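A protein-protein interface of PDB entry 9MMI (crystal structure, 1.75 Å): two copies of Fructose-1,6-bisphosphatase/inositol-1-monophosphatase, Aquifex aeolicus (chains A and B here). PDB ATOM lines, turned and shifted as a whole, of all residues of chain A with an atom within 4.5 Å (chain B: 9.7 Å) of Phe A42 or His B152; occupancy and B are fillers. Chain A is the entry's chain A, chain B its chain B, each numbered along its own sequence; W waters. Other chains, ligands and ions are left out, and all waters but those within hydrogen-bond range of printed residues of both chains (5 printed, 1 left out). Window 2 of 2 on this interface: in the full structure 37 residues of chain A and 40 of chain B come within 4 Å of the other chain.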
ATOM      1  N   LYS A  31     -22.801 -18.186   9.080  1.00  0.00           N
ATOM      2  CA  LYS A  31     -22.772 -17.484   7.808  1.00  0.00           C
ATOM      3  C   LYS A  31     -22.844 -15.990   7.995  1.00  0.00           C
ATOM      4  O   LYS A  31     -22.247 -15.246   7.211  1.00  0.00           O
ATOM      5  CB  LYS A  31     -23.924 -17.967   6.935  1.00  0.00           C
ATOM      6  CG  LYS A  31     -23.677 -19.327   6.332  1.00  0.00           C
ATOM      7  CD  LYS A  31     -24.638 -19.542   5.181  1.00  0.00           C
ATOM      8  CE  LYS A  31     -24.506 -20.920   4.607  1.00  0.00           C
ATOM      9  NZ  LYS A  31     -25.675 -21.187   3.782  1.00  0.00           N
ATOM     10  N   ILE A  34     -19.386 -14.322   8.160  1.00  0.00           N
ATOM     11  CA  ILE A  34     -18.399 -14.582   7.109  1.00  0.00           C
ATOM     12  C   ILE A  34     -18.418 -13.422   6.128  1.00  0.00           C
ATOM     13  O   ILE A  34     -19.473 -13.105   5.558  1.00  0.00           O
ATOM     14  CB  ILE A  34     -18.687 -15.908   6.393  1.00  0.00           C
ATOM     15  CG1 ILE A  34     -18.670 -17.097   7.368  1.00  0.00           C
ATOM     16  CG2 ILE A  34     -17.689 -16.143   5.227  1.00  0.00           C
ATOM     17  CD1 ILE A  34     -19.260 -18.373   6.769  1.00  0.00           C
ATOM     18  N   GLU A  35     -17.262 -12.799   5.917  1.00  0.00           N
ATOM     19  CA  GLU A  35     -17.087 -11.847   4.828  1.00  0.00           C
ATOM     20  C   GLU A  35     -16.458 -12.562   3.639  1.00  0.00           C
ATOM     21  O   GLU A  35     -15.562 -13.386   3.816  1.00  0.00           O
ATOM     22  CB  GLU A  35     -16.190 -10.670   5.197  1.00  0.00           C
ATOM     23  CG  GLU A  35     -16.467  -9.993   6.516  1.00  0.00           C
ATOM     24  CD  GLU A  35     -15.358  -9.018   6.894  1.00  0.00           C
ATOM     25  OE1 GLU A  35     -14.557  -8.644   6.001  1.00  0.00           O
ATOM     26  OE2 GLU A  35     -15.280  -8.640   8.084  1.00  0.00           O
ATOM     27  N   LYS A  40     -13.649 -16.579  -4.008  1.00  0.00           N
ATOM     28  CA  LYS A  40     -13.924 -17.759  -3.209  1.00  0.00           C
ATOM     29  C   LYS A  40     -13.441 -17.699  -1.766  1.00  0.00           C
ATOM     30  O   LYS A  40     -13.744 -18.631  -1.011  1.00  0.00           O
ATOM     31  CB  LYS A  40     -13.299 -19.021  -3.840  1.00  0.00           C
ATOM     32  CG  LYS A  40     -13.744 -19.343  -5.252  1.00  0.00           C
ATOM     33  CD  LYS A  40     -15.166 -19.918  -5.317  1.00  0.00           C
ATOM     34  CE  LYS A  40     -15.221 -21.345  -4.793  1.00  0.00           C
ATOM     35  NZ  LYS A  40     -14.728 -22.408  -5.733  1.00  0.00           N
ATOM     36  N   ASP A  41     -12.699 -16.670  -1.364  1.00  0.00           N
ATOM     37  CA  ASP A  41     -12.088 -16.670  -0.045  1.00  0.00           C
ATOM     38  C   ASP A  41     -13.045 -16.117   1.006  1.00  0.00           C
ATOM     39  O   ASP A  41     -13.853 -15.234   0.729  1.00  0.00           O
ATOM     40  CB  ASP A  41     -10.784 -15.880  -0.044  1.00  0.00           C
ATOM     41  CG  ASP A  41      -9.684 -16.573  -0.837  1.00  0.00           C
ATOM     42  OD1 ASP A  41      -9.525 -17.802  -0.686  1.00  0.00           O
ATOM     43  OD2 ASP A  41      -8.991 -15.888  -1.623  1.00  0.00           O
ATOM     44  N   PHE A  42     -12.913 -16.635   2.221  1.00  0.00           N
ATOM     45  CA  PHE A  42     -13.711 -16.216   3.371  1.00  0.00           C
ATOM     46  C   PHE A  42     -12.777 -15.684   4.458  1.00  0.00           C
ATOM     47  O   PHE A  42     -11.629 -16.116   4.565  1.00  0.00           O
ATOM     48  CB  PHE A  42     -14.485 -17.388   3.981  1.00  0.00           C
ATOM     49  CG  PHE A  42     -15.572 -17.934   3.114  1.00  0.00           C
ATOM     50  CD1 PHE A  42     -16.155 -17.154   2.157  1.00  0.00           C
ATOM     51  CD2 PHE A  42     -16.000 -19.246   3.270  1.00  0.00           C
ATOM     52  CE1 PHE A  42     -17.171 -17.658   1.348  1.00  0.00           C
ATOM     53  CE2 PHE A  42     -17.013 -19.744   2.479  1.00  0.00           C
ATOM     54  CZ  PHE A  42     -17.586 -18.940   1.518  1.00  0.00           C
ATOM     55  N   VAL A  43     -13.294 -14.749   5.255  1.00  0.00           N
ATOM     56  CA  VAL A  43     -12.615 -14.294   6.470  1.00  0.00           C
ATOM     57  C   VAL A  43     -13.697 -13.953   7.477  1.00  0.00           C
ATOM     58  O   VAL A  43     -14.820 -13.619   7.103  1.00  0.00           O
ATOM     59  CB  VAL A  43     -11.685 -13.092   6.200  1.00  0.00           C
ATOM     60  CG1 VAL A  43     -12.459 -11.862   5.777  1.00  0.00           C
ATOM     61  CG2 VAL A  43     -10.793 -12.803   7.436  1.00  0.00           C
ATOM     62  N   THR A  91      -8.914 -21.601   6.969  1.00  0.00           N
ATOM     63  CA  THR A  91     -10.161 -20.944   7.309  1.00  0.00           C
ATOM     64  C   THR A  91     -11.381 -21.767   6.898  1.00  0.00           C
ATOM     65  O   THR A  91     -12.352 -21.893   7.665  1.00  0.00           O
ATOM     66  CB  THR A  91     -10.212 -19.564   6.644  1.00  0.00           C
ATOM     67  OG1 THR A  91      -9.169 -18.750   7.158  1.00  0.00           O
ATOM     68  CG2 THR A  91     -11.474 -18.892   6.933  1.00  0.00           C
ATOM     69  N   LYS A  92     -11.389 -22.305   5.667  1.00  0.00           N
ATOM     70  CA  LYS A  92     -12.580 -23.066   5.258  1.00  0.00           C
ATOM     71  C   LYS A  92     -12.790 -24.303   6.128  1.00  0.00           C
ATOM     72  O   LYS A  92     -13.933 -24.582   6.544  1.00  0.00           O
ATOM     73  CB  LYS A  92     -12.461 -23.428   3.786  1.00  0.00           C
ATOM     74  CG  LYS A  92     -12.569 -22.131   2.930  1.00  0.00           C
ATOM     75  CD  LYS A  92     -12.421 -22.406   1.458  1.00  0.00           C
ATOM     76  CE  LYS A  92     -12.861 -21.237   0.557  1.00  0.00           C
ATOM     77  NZ  LYS A  92     -14.010 -20.572   1.123  1.00  0.00           N
ATOM     78  N   ILE A  95     -14.230 -23.116   9.582  1.00  0.00           N
ATOM     79  CA  ILE A  95     -15.646 -22.775   9.531  1.00  0.00           C
ATOM     80  C   ILE A  95     -16.507 -24.035   9.433  1.00  0.00           C
ATOM     81  O   ILE A  95     -17.588 -24.097  10.029  1.00  0.00           O
ATOM     82  CB  ILE A  95     -15.895 -21.810   8.356  1.00  0.00           C
ATOM     83  CG1 ILE A  95     -15.195 -20.466   8.656  1.00  0.00           C
ATOM     84  CG2 ILE A  95     -17.377 -21.640   8.073  1.00  0.00           C
ATOM     85  CD1 ILE A  95     -15.121 -19.532   7.499  1.00  0.00           C
ATOM     86  N   ASN A  96     -16.045 -25.044   8.700  1.00  0.00           N
ATOM     87  CA  ASN A  96     -16.791 -26.291   8.537  1.00  0.00           C
ATOM     88  C   ASN A  96     -16.696 -27.198   9.767  1.00  0.00           C
ATOM     89  O   ASN A  96     -17.511 -28.112   9.913  1.00  0.00           O
ATOM     90  CB  ASN A  96     -16.302 -27.080   7.346  1.00  0.00           C
ATOM     91  CG  ASN A  96     -16.805 -26.514   6.040  1.00  0.00           C
ATOM     92  OD1 ASN A  96     -17.877 -25.935   6.001  1.00  0.00           O
ATOM     93  ND2 ASN A  96     -16.016 -26.656   4.971  1.00  0.00           N
ATOM     94  N   LYS B 145     -25.487 -31.255   7.610  1.00  0.00           N
ATOM     95  CA  LYS B 145     -25.637 -29.773   7.614  1.00  0.00           C
ATOM     96  C   LYS B 145     -26.753 -29.352   6.655  1.00  0.00           C
ATOM     97  O   LYS B 145     -27.034 -30.099   5.737  1.00  0.00           O
ATOM     98  CB  LYS B 145     -24.335 -29.050   7.259  1.00  0.00           C
ATOM     99  CG  LYS B 145     -23.671 -29.419   5.947  1.00  0.00           C
ATOM    100  CD  LYS B 145     -22.181 -29.182   6.016  1.00  0.00           C
ATOM    101  CE  LYS B 145     -21.837 -27.725   6.237  1.00  0.00           C
ATOM    102  NZ  LYS B 145     -20.382 -27.485   6.116  1.00  0.00           N
ATOM    103  N   ASP B 146     -27.362 -28.186   6.889  1.00  0.00           N
ATOM    104  CA  ASP B 146     -28.485 -27.718   6.066  1.00  0.00           C
ATOM    105  C   ASP B 146     -28.090 -26.944   4.807  1.00  0.00           C
ATOM    106  O   ASP B 146     -28.944 -26.693   3.938  1.00  0.00           O
ATOM    107  CB  ASP B 146     -29.398 -26.803   6.892  1.00  0.00           C
ATOM    108  CG  ASP B 146     -30.140 -27.541   7.956  1.00  0.00           C
ATOM    109  OD1 ASP B 146     -30.494 -28.714   7.707  1.00  0.00           O
ATOM    110  OD2 ASP B 146     -30.345 -26.961   9.048  1.00  0.00           O
ATOM    111  N   ASN B 147     -26.854 -26.544   4.697  1.00  0.00           N
ATOM    112  CA  ASN B 147     -26.452 -25.590   3.681  1.00  0.00           C
ATOM    113  C   ASN B 147     -26.802 -26.029   2.257  1.00  0.00           C
ATOM    114  O   ASN B 147     -26.588 -27.177   1.863  1.00  0.00           O
ATOM    115  CB  ASN B 147     -24.951 -25.399   3.836  1.00  0.00           C
ATOM    116  CG  ASN B 147     -24.370 -24.583   2.737  1.00  0.00           C
ATOM    117  OD1 ASN B 147     -24.703 -23.396   2.595  1.00  0.00           O
ATOM    118  ND2 ASN B 147     -23.559 -25.225   1.899  1.00  0.00           N
ATOM    119  N   GLU B 148     -27.272 -25.071   1.480  1.00  0.00           N
ATOM    120  CA  GLU B 148     -27.525 -25.261   0.055  1.00  0.00           C
ATOM    121  C   GLU B 148     -26.633 -24.390  -0.810  1.00  0.00           C
ATOM    122  O   GLU B 148     -26.673 -24.515  -2.041  1.00  0.00           O
ATOM    123  CB  GLU B 148     -28.994 -24.972  -0.249  1.00  0.00           C
ATOM    124  CG  GLU B 148     -29.905 -25.890   0.544  1.00  0.00           C
ATOM    125  CD  GLU B 148     -31.292 -25.945  -0.002  1.00  0.00           C
ATOM    126  OE1 GLU B 148     -31.519 -25.465  -1.129  1.00  0.00           O
ATOM    127  OE2 GLU B 148     -32.176 -26.474   0.702  1.00  0.00           O
ATOM    128  N   SER B 149     -25.852 -23.501  -0.198  1.00  0.00           N
ATOM    129  CA  SER B 149     -24.993 -22.578  -0.917  1.00  0.00           C
ATOM    130  C   SER B 149     -23.728 -23.283  -1.366  1.00  0.00           C
ATOM    131  O   SER B 149     -22.935 -23.742  -0.528  1.00  0.00           O
ATOM    132  CB  SER B 149     -24.632 -21.394  -0.017  1.00  0.00           C
ATOM    133  OG  SER B 149     -23.732 -20.571  -0.721  1.00  0.00           O
ATOM    134  N   LEU B 150     -23.523 -23.388  -2.682  1.00  0.00           N
ATOM    135  CA  LEU B 150     -22.360 -24.133  -3.152  1.00  0.00           C
ATOM    136  C   LEU B 150     -21.062 -23.498  -2.657  1.00  0.00           C
ATOM    137  O   LEU B 150     -20.132 -24.213  -2.299  1.00  0.00           O
ATOM    138  CB  LEU B 150     -22.377 -24.237  -4.679  1.00  0.00           C
ATOM    139  CG  LEU B 150     -23.574 -25.004  -5.226  1.00  0.00           C
ATOM    140  CD1 LEU B 150     -23.453 -25.106  -6.768  1.00  0.00           C
ATOM    141  CD2 LEU B 150     -23.702 -26.393  -4.596  1.00  0.00           C
ATOM    142  N   LYS B 151     -20.973 -22.160  -2.670  1.00  0.00           N
ATOM    143  CA  LYS B 151     -19.713 -21.521  -2.317  1.00  0.00           C
ATOM    144  C   LYS B 151     -19.368 -21.711  -0.855  1.00  0.00           C
ATOM    145  O   LYS B 151     -18.199 -21.592  -0.477  1.00  0.00           O
ATOM    146  CB  LYS B 151     -19.774 -20.006  -2.595  1.00  0.00           C
ATOM    147  CG  LYS B 151     -20.023 -19.577  -4.032  1.00  0.00           C
ATOM    148  CD  LYS B 151     -21.283 -20.222  -4.631  1.00  0.00           C
ATOM    149  CE  LYS B 151     -22.521 -19.937  -3.825  1.00  0.00           C
ATOM    150  NZ  LYS B 151     -23.520 -20.825  -4.269  1.00  0.00           N
ATOM    151  N   HIS B 152     -20.356 -22.025  -0.019  1.00  0.00           N
ATOM    152  CA  HIS B 152     -20.091 -22.363   1.365  1.00  0.00           C
ATOM    153  C   HIS B 152     -19.868 -23.847   1.604  1.00  0.00           C
ATOM    154  O   HIS B 152     -19.385 -24.218   2.674  1.00  0.00           O
ATOM    155  CB  HIS B 152     -21.251 -21.887   2.234  1.00  0.00           C
ATOM    156  CG  HIS B 152     -21.377 -20.405   2.311  1.00  0.00           C
ATOM    157  ND1 HIS B 152     -22.178 -19.687   1.448  1.00  0.00           N
ATOM    158  CD2 HIS B 152     -20.803 -19.500   3.147  1.00  0.00           C
ATOM    159  CE1 HIS B 152     -22.098 -18.401   1.751  1.00  0.00           C
ATOM    160  NE2 HIS B 152     -21.274 -18.259   2.772  1.00  0.00           N
ATOM    161  N   ALA B 153     -20.153 -24.683   0.624  1.00  0.00           N
ATOM    162  CA  ALA B 153     -20.061 -26.123   0.811  1.00  0.00           C
ATOM    163  C   ALA B 153     -18.622 -26.604   0.840  1.00  0.00           C
ATOM    164  O   ALA B 153     -17.740 -26.056   0.172  1.00  0.00           O
ATOM    165  CB  ALA B 153     -20.791 -26.839  -0.315  1.00  0.00           C
ATOM    166  N   GLY B 154     -18.399 -27.648   1.640  1.00  0.00           N
ATOM    167  CA  GLY B 154     -17.203 -28.464   1.607  1.00  0.00           C
ATOM    168  C   GLY B 154     -17.549 -29.862   1.123  1.00  0.00           C
ATOM    169  O   GLY B 154     -18.559 -30.441   1.570  1.00  0.00           O
ATOM    170  N   VAL B 155     -16.694 -30.411   0.255  1.00  0.00           N
ATOM    171  CA  VAL B 155     -16.891 -31.725  -0.341  1.00  0.00           C
ATOM    172  C   VAL B 155     -15.647 -32.573  -0.121  1.00  0.00           C
ATOM    173  O   VAL B 155     -14.508 -32.114  -0.346  1.00  0.00           O
ATOM    174  CB  VAL B 155     -17.233 -31.631  -1.847  1.00  0.00           C
ATOM    175  CG1 VAL B 155     -17.319 -32.994  -2.429  1.00  0.00           C
ATOM    176  CG2 VAL B 155     -18.514 -30.839  -2.070  1.00  0.00           C
ATOM    177  N   TYR B 179     -14.727 -26.028  -9.080  1.00  0.00           N
ATOM    178  CA  TYR B 179     -14.944 -24.658  -9.522  1.00  0.00           C
ATOM    179  C   TYR B 179     -16.044 -23.975  -8.714  1.00  0.00           C
ATOM    180  O   TYR B 179     -15.977 -22.771  -8.474  1.00  0.00           O
ATOM    181  CB  TYR B 179     -15.284 -24.633 -11.010  1.00  0.00           C
ATOM    182  CG  TYR B 179     -15.242 -23.233 -11.566  1.00  0.00           C
ATOM    183  CD1 TYR B 179     -14.017 -22.625 -11.847  1.00  0.00           C
ATOM    184  CD2 TYR B 179     -16.398 -22.495 -11.720  1.00  0.00           C
ATOM    185  CE1 TYR B 179     -13.952 -21.315 -12.309  1.00  0.00           C
ATOM    186  CE2 TYR B 179     -16.331 -21.187 -12.170  1.00  0.00           C
ATOM    187  CZ  TYR B 179     -15.108 -20.609 -12.460  1.00  0.00           C
ATOM    188  OH  TYR B 179     -15.026 -19.305 -12.928  1.00  0.00           O
ATOM    189  N   GLU B 180     -17.083 -24.716  -8.331  1.00  0.00           N
ATOM    190  CA  GLU B 180     -18.254 -24.146  -7.698  1.00  0.00           C
ATOM    191  C   GLU B 180     -18.249 -24.155  -6.170  1.00  0.00           C
ATOM    192  O   GLU B 180     -18.855 -23.264  -5.547  1.00  0.00           O
ATOM    193  CB  GLU B 180     -19.529 -24.878  -8.154  1.00  0.00           C
ATOM    194  CG  GLU B 180     -19.834 -24.884  -9.638  1.00  0.00           C
ATOM    195  CD  GLU B 180     -19.858 -23.530 -10.308  1.00  0.00           C
ATOM    196  OE1 GLU B 180     -20.095 -22.506  -9.653  1.00  0.00           O
ATOM    197  OE2 GLU B 180     -19.707 -23.497 -11.541  1.00  0.00           O
ATOM    198  N   VAL B 181     -17.660 -25.160  -5.535  1.00  0.00           N
ATOM    199  CA  VAL B 181     -17.821 -25.320  -4.084  1.00  0.00           C
ATOM    200  C   VAL B 181     -16.734 -24.568  -3.344  1.00  0.00           C
ATOM    201  O   VAL B 181     -15.686 -24.201  -3.881  1.00  0.00           O
ATOM    202  CB  VAL B 181     -17.903 -26.809  -3.650  1.00  0.00           C
ATOM    203  CG1 VAL B 181     -19.078 -27.469  -4.397  1.00  0.00           C
ATOM    204  CG2 VAL B 181     -16.597 -27.511  -3.796  1.00  0.00           C
ATOM    205  N   GLY B 182     -17.000 -24.324  -2.064  1.00  0.00           N
ATOM    206  CA  GLY B 182     -16.034 -23.617  -1.250  1.00  0.00           C
ATOM    207  C   GLY B 182     -14.732 -24.355  -1.041  1.00  0.00           C
ATOM    208  O   GLY B 182     -13.662 -23.741  -1.059  1.00  0.00           O
ATOM    209  N   SER B 183     -14.788 -25.660  -0.769  1.00  0.00           N
ATOM    210  CA  SER B 183     -13.555 -26.415  -0.581  1.00  0.00           C
ATOM    211  C   SER B 183     -13.780 -27.875  -0.935  1.00  0.00           C
ATOM    212  O   SER B 183     -14.906 -28.410  -0.858  1.00  0.00           O
ATOM    213  CB  SER B 183     -13.030 -26.270   0.857  1.00  0.00           C
ATOM    214  OG  SER B 183     -13.988 -26.786   1.739  1.00  0.00           O
ATOM    215  N   MET B 184     -12.709 -28.494  -1.368  1.00  0.00           N
ATOM    216  CA  MET B 184     -12.631 -29.939  -1.569  1.00  0.00           C
ATOM    217  C   MET B 184     -11.463 -30.496  -0.805  1.00  0.00           C
ATOM    218  O   MET B 184     -10.355 -29.938  -0.847  1.00  0.00           O
ATOM    219  CB  MET B 184     -12.529 -30.342  -3.035  1.00  0.00           C
ATOM    220  CG  MET B 184     -13.467 -29.579  -3.879  1.00  0.00           C
ATOM    221  SD  MET B 184     -13.999 -30.408  -5.396  1.00  0.00           S
ATOM    222  CE  MET B 184     -14.259 -32.160  -5.104  1.00  0.00           C
ATOM    223  N   ARG B 185     -11.697 -31.620  -0.137  1.00  0.00           N
ATOM    224  CA  ARG B 185     -10.679 -32.215   0.712  1.00  0.00           C
ATOM    225  C   ARG B 185     -10.577 -33.701   0.437  1.00  0.00           C
ATOM    226  O   ARG B 185     -11.577 -34.380   0.182  1.00  0.00           O
ATOM    227  CB  ARG B 185     -11.008 -31.964   2.218  1.00  0.00           C
ATOM    228  CG  ARG B 185     -11.084 -30.474   2.611  1.00  0.00           C
ATOM    229  CD  ARG B 185      -9.714 -29.803   2.556  1.00  0.00           C
ATOM    230  NE  ARG B 185      -9.861 -28.371   2.800  1.00  0.00           N
ATOM    231  CZ  ARG B 185      -9.736 -27.405   1.910  1.00  0.00           C
ATOM    232  NH1 ARG B 185      -9.500 -27.647   0.624  1.00  0.00           N
ATOM    233  NH2 ARG B 185      -9.882 -26.152   2.314  1.00  0.00           N
ATOM    234  N   GLY B 200     -22.073 -33.436   9.859  1.00  0.00           N
ATOM    235  CA  GLY B 200     -22.348 -32.053   9.487  1.00  0.00           C
ATOM    236  C   GLY B 200     -21.108 -31.209   9.248  1.00  0.00           C
ATOM    237  O   GLY B 200     -21.215 -29.978   9.269  1.00  0.00           O
ATOM    238  N   ILE B 201     -19.961 -31.836   9.036  1.00  0.00           N
ATOM    239  CA  ILE B 201     -18.728 -31.118   8.725  1.00  0.00           C
ATOM    240  C   ILE B 201     -18.670 -30.802   7.227  1.00  0.00           C
ATOM    241  O   ILE B 201     -18.531 -29.639   6.804  1.00  0.00           O
ATOM    242  CB  ILE B 201     -17.498 -31.918   9.181  1.00  0.00           C
ATOM    243  CG1 ILE B 201     -17.499 -32.120  10.700  1.00  0.00           C
ATOM    244  CG2 ILE B 201     -16.184 -31.175   8.727  1.00  0.00           C
ATOM    245  CD1 ILE B 201     -16.430 -33.068  11.166  1.00  0.00           C
ATOM    246  N   PHE B 202     -18.846 -31.815   6.408  1.00  0.00           N
ATOM    247  CA  PHE B 202     -18.838 -31.660   4.955  1.00  0.00           C
ATOM    248  C   PHE B 202     -20.242 -31.830   4.445  1.00  0.00           C
ATOM    249  O   PHE B 202     -21.027 -32.606   5.008  1.00  0.00           O
ATOM    250  CB  PHE B 202     -17.888 -32.647   4.328  1.00  0.00           C
ATOM    251  CG  PHE B 202     -16.436 -32.352   4.685  1.00  0.00           C
ATOM    252  CD1 PHE B 202     -15.803 -31.250   4.141  1.00  0.00           C
ATOM    253  CD2 PHE B 202     -15.747 -33.130   5.574  1.00  0.00           C
ATOM    254  CE1 PHE B 202     -14.476 -30.970   4.452  1.00  0.00           C
ATOM    255  CE2 PHE B 202     -14.432 -32.859   5.875  1.00  0.00           C
ATOM    256  CZ  PHE B 202     -13.810 -31.768   5.345  1.00  0.00           C
ATOM    257  N   ASP B 203     -20.584 -31.036   3.425  1.00  0.00           N
ATOM    258  CA  ASP B 203     -21.908 -31.097   2.842  1.00  0.00           C
ATOM    259  C   ASP B 203     -22.083 -32.234   1.830  1.00  0.00           C
ATOM    260  O   ASP B 203     -23.212 -32.664   1.571  1.00  0.00           O
ATOM    261  CB  ASP B 203     -22.228 -29.796   2.060  1.00  0.00           C
ATOM    262  CG  ASP B 203     -21.844 -28.508   2.768  1.00  0.00           C
ATOM    263  OD1 ASP B 203     -20.664 -28.293   3.218  1.00  0.00           O
ATOM    264  OD2 ASP B 203     -22.746 -27.668   2.803  1.00  0.00           O
ATOM    265  N   GLY B 204     -20.996 -32.703   1.222  1.00  0.00           N
ATOM    266  CA  GLY B 204     -21.076 -33.704   0.181  1.00  0.00           C
ATOM    267  C   GLY B 204     -19.818 -34.526   0.095  1.00  0.00           C
ATOM    268  O   GLY B 204     -18.778 -34.176   0.653  1.00  0.00           O
ATOM    269  N   ASN B 245     -25.860 -33.854   1.977  1.00  0.00           N
ATOM    270  CA  ASN B 245     -27.207 -33.336   2.158  1.00  0.00           C
ATOM    271  C   ASN B 245     -27.869 -33.297   0.781  1.00  0.00           C
ATOM    272  O   ASN B 245     -27.260 -33.653  -0.260  1.00  0.00           O
ATOM    273  CB  ASN B 245     -27.195 -31.992   2.893  1.00  0.00           C
ATOM    274  CG  ASN B 245     -26.474 -30.904   2.122  1.00  0.00           C
ATOM    275  OD1 ASN B 245     -26.345 -30.970   0.882  1.00  0.00           O
ATOM    276  ND2 ASN B 245     -26.069 -29.856   2.836  1.00  0.00           N
ATOM    277  N   LEU B 248     -26.210 -30.853  -1.995  1.00  0.00           N
ATOM    278  CA  LEU B 248     -24.900 -31.228  -2.525  1.00  0.00           C
ATOM    279  C   LEU B 248     -24.936 -32.590  -3.192  1.00  0.00           C
ATOM    280  O   LEU B 248     -24.253 -32.790  -4.196  1.00  0.00           O
ATOM    281  CB  LEU B 248     -23.819 -31.173  -1.462  1.00  0.00           C
ATOM    282  CG  LEU B 248     -23.140 -29.800  -1.425  1.00  0.00           C
ATOM    283  CD1 LEU B 248     -22.363 -29.479  -2.716  1.00  0.00           C
ATOM    284  CD2 LEU B 248     -24.158 -28.705  -1.159  1.00  0.00           C
HETATM  285  O   HOH W   1     -28.183 -22.473   2.554  1.00  0.00           O
HETATM  286  O   HOH W   2     -18.470 -23.427   4.996  1.00  0.00           O
HETATM  287  O   HOH W   3     -16.019 -24.940   2.387  1.00  0.00           O
HETATM  288  O   HOH W   4     -13.288 -27.566   4.360  1.00  0.00           O
HETATM  289  O   HOH W   5     -21.697 -15.777   4.129  1.00  0.00           O
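The side-chain amino group of Lys A40 lies within hydrogen-bond range of the backbone carbonyl oxygen of Tyr B179 (3.0 Å).
The side-chain amino group (NZ) of Lys A40 sits at hydrogen-bond distance from the backbone carbonyl oxygen (O) of Val B181 (2.8 Å).
NZ of Lys B145 is in hydrogen-bond range of OD1 of Asn A96 (2.9 Å).
OD1 of Asn B147 lies within hydrogen-bond range of NZ of Lys A31, 2.7 Å away.
The side-chain amino group of Lys A92 lies within hydrogen-bond range of the backbone carbonyl oxygen of Lys A40 (2.9 Å).
N of Gly B204 lies within hydrogen-bond range of O of Gly B154.
O of Leu B150 is in hydrogen-bond range of N of Gly B182.
The side-chain carboxylate (OD2) of Asp B203 is in hydrogen-bond range of the side-chain amide nitrogen (ND2) of Asn B147, 2.7 Å away.
The backbone carbonyl oxygen (O) of Lys A92 lies within hydrogen-bond range of the side-chain amide nitrogen (ND2) of Asn A96, 3.3 Å away.
The side-chain amino group (NZ) of Lys B145 is in salt-bridge range of the side-chain carboxylate (OD1) of Asp B203 (3.0 Å).
Lys A31 touches Ser B149.
Lys A31 touches His B152 (CE to CG, 3.9 Å).
Lys A40 touches Glu B180 (NZ to C, 3.95 Å).
CZ of Phe A42 touches O of Lys B151, at 3.4 Å.
His B152 touches Phe A42 (CD2 to CZ, 3.6 Å).
Lys A92 touches Gly B182 (CE to O, 3.1 Å).
Ser B183 touches Lys A92 (CB to CD, 3.96 Å).
ND2 of Asn A96 touches CA of Gly B154, at 3.999 Å.
Ser B183 touches Asn A96 (OG to ND2, 3.8 Å).
Ile B201 touches Asn A96.
Phe A42 touches just these residues of chain B: Lys B151 and His B152.
His B152 touches just these residues of chain A: Lys A31 and Phe A42.
No residue of chain B comes within 4 Å of Asp A41.
No residue of chain B comes within 4 Å of Val A43.
Of the printed residues of chain B, Lys A40 touches Tyr B179 (3.0 Å), Glu B180 (3.95 Å) and Val B181 (2.8 Å).
Of the printed residues of chain A, Ile B201 touches Asn A96 (3.4 Å).
Of the printed residues of chain B, Lys A31 touches Asn B147, Ser B149 and His B152.
Of the printed residues of chain A, Tyr B179 touches Lys A40.
Printed residues of chain A within 4 Å of Lys B145: Asn A96.
Asp B203 touches none of the printed residues of chain A.
The nearest residue of chain B that does not touch Phe A42 is Gly B182 (5.5 Å).
The nearest residue of chain A that does not touch His B152 is Asn A96 (4.04 Å).
The nearest printed residue of chain A that does not touch Asn B147 is Asn A96 (7.0 Å).
Of the 25 printed residues of chain B, 12 touch a printed residue of chain A.
Printed residues of chain A that touch a printed residue of chain B: Lys A31, Lys A40, Phe A42, Lys A92 and Asn A96.
No position is printed for both chains.
Of the 14 pairs that touch across the chains among the printed residues, none has its exchanged pair printed and touching as well.
Water W2 lies within hydrogen-bond range of O of His B152 and OD1 of Asn A96.
Water W3 lies within hydrogen-bond range of the side-chain hydroxyl of Ser B183, the backbone carbonyl oxygen of Ala B153, the side-chain amide nitrogen of Asn A96 and the backbone carbonyl oxygen of His B152.
Water W4 lies within hydrogen-bond range of the side-chain hydroxyl of Ser B183 (2.8 Å) and the side-chain amide nitrogen of Asn A96 (2.9 Å).
Water W5 bridges NE2 of His B152 (2.9 Å) and O of Lys A31 (3.2 Å).
Water W1 lies within hydrogen-bond range of N of Glu B148 (3.0 Å) and NZ of Lys A31 (3.1 Å).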
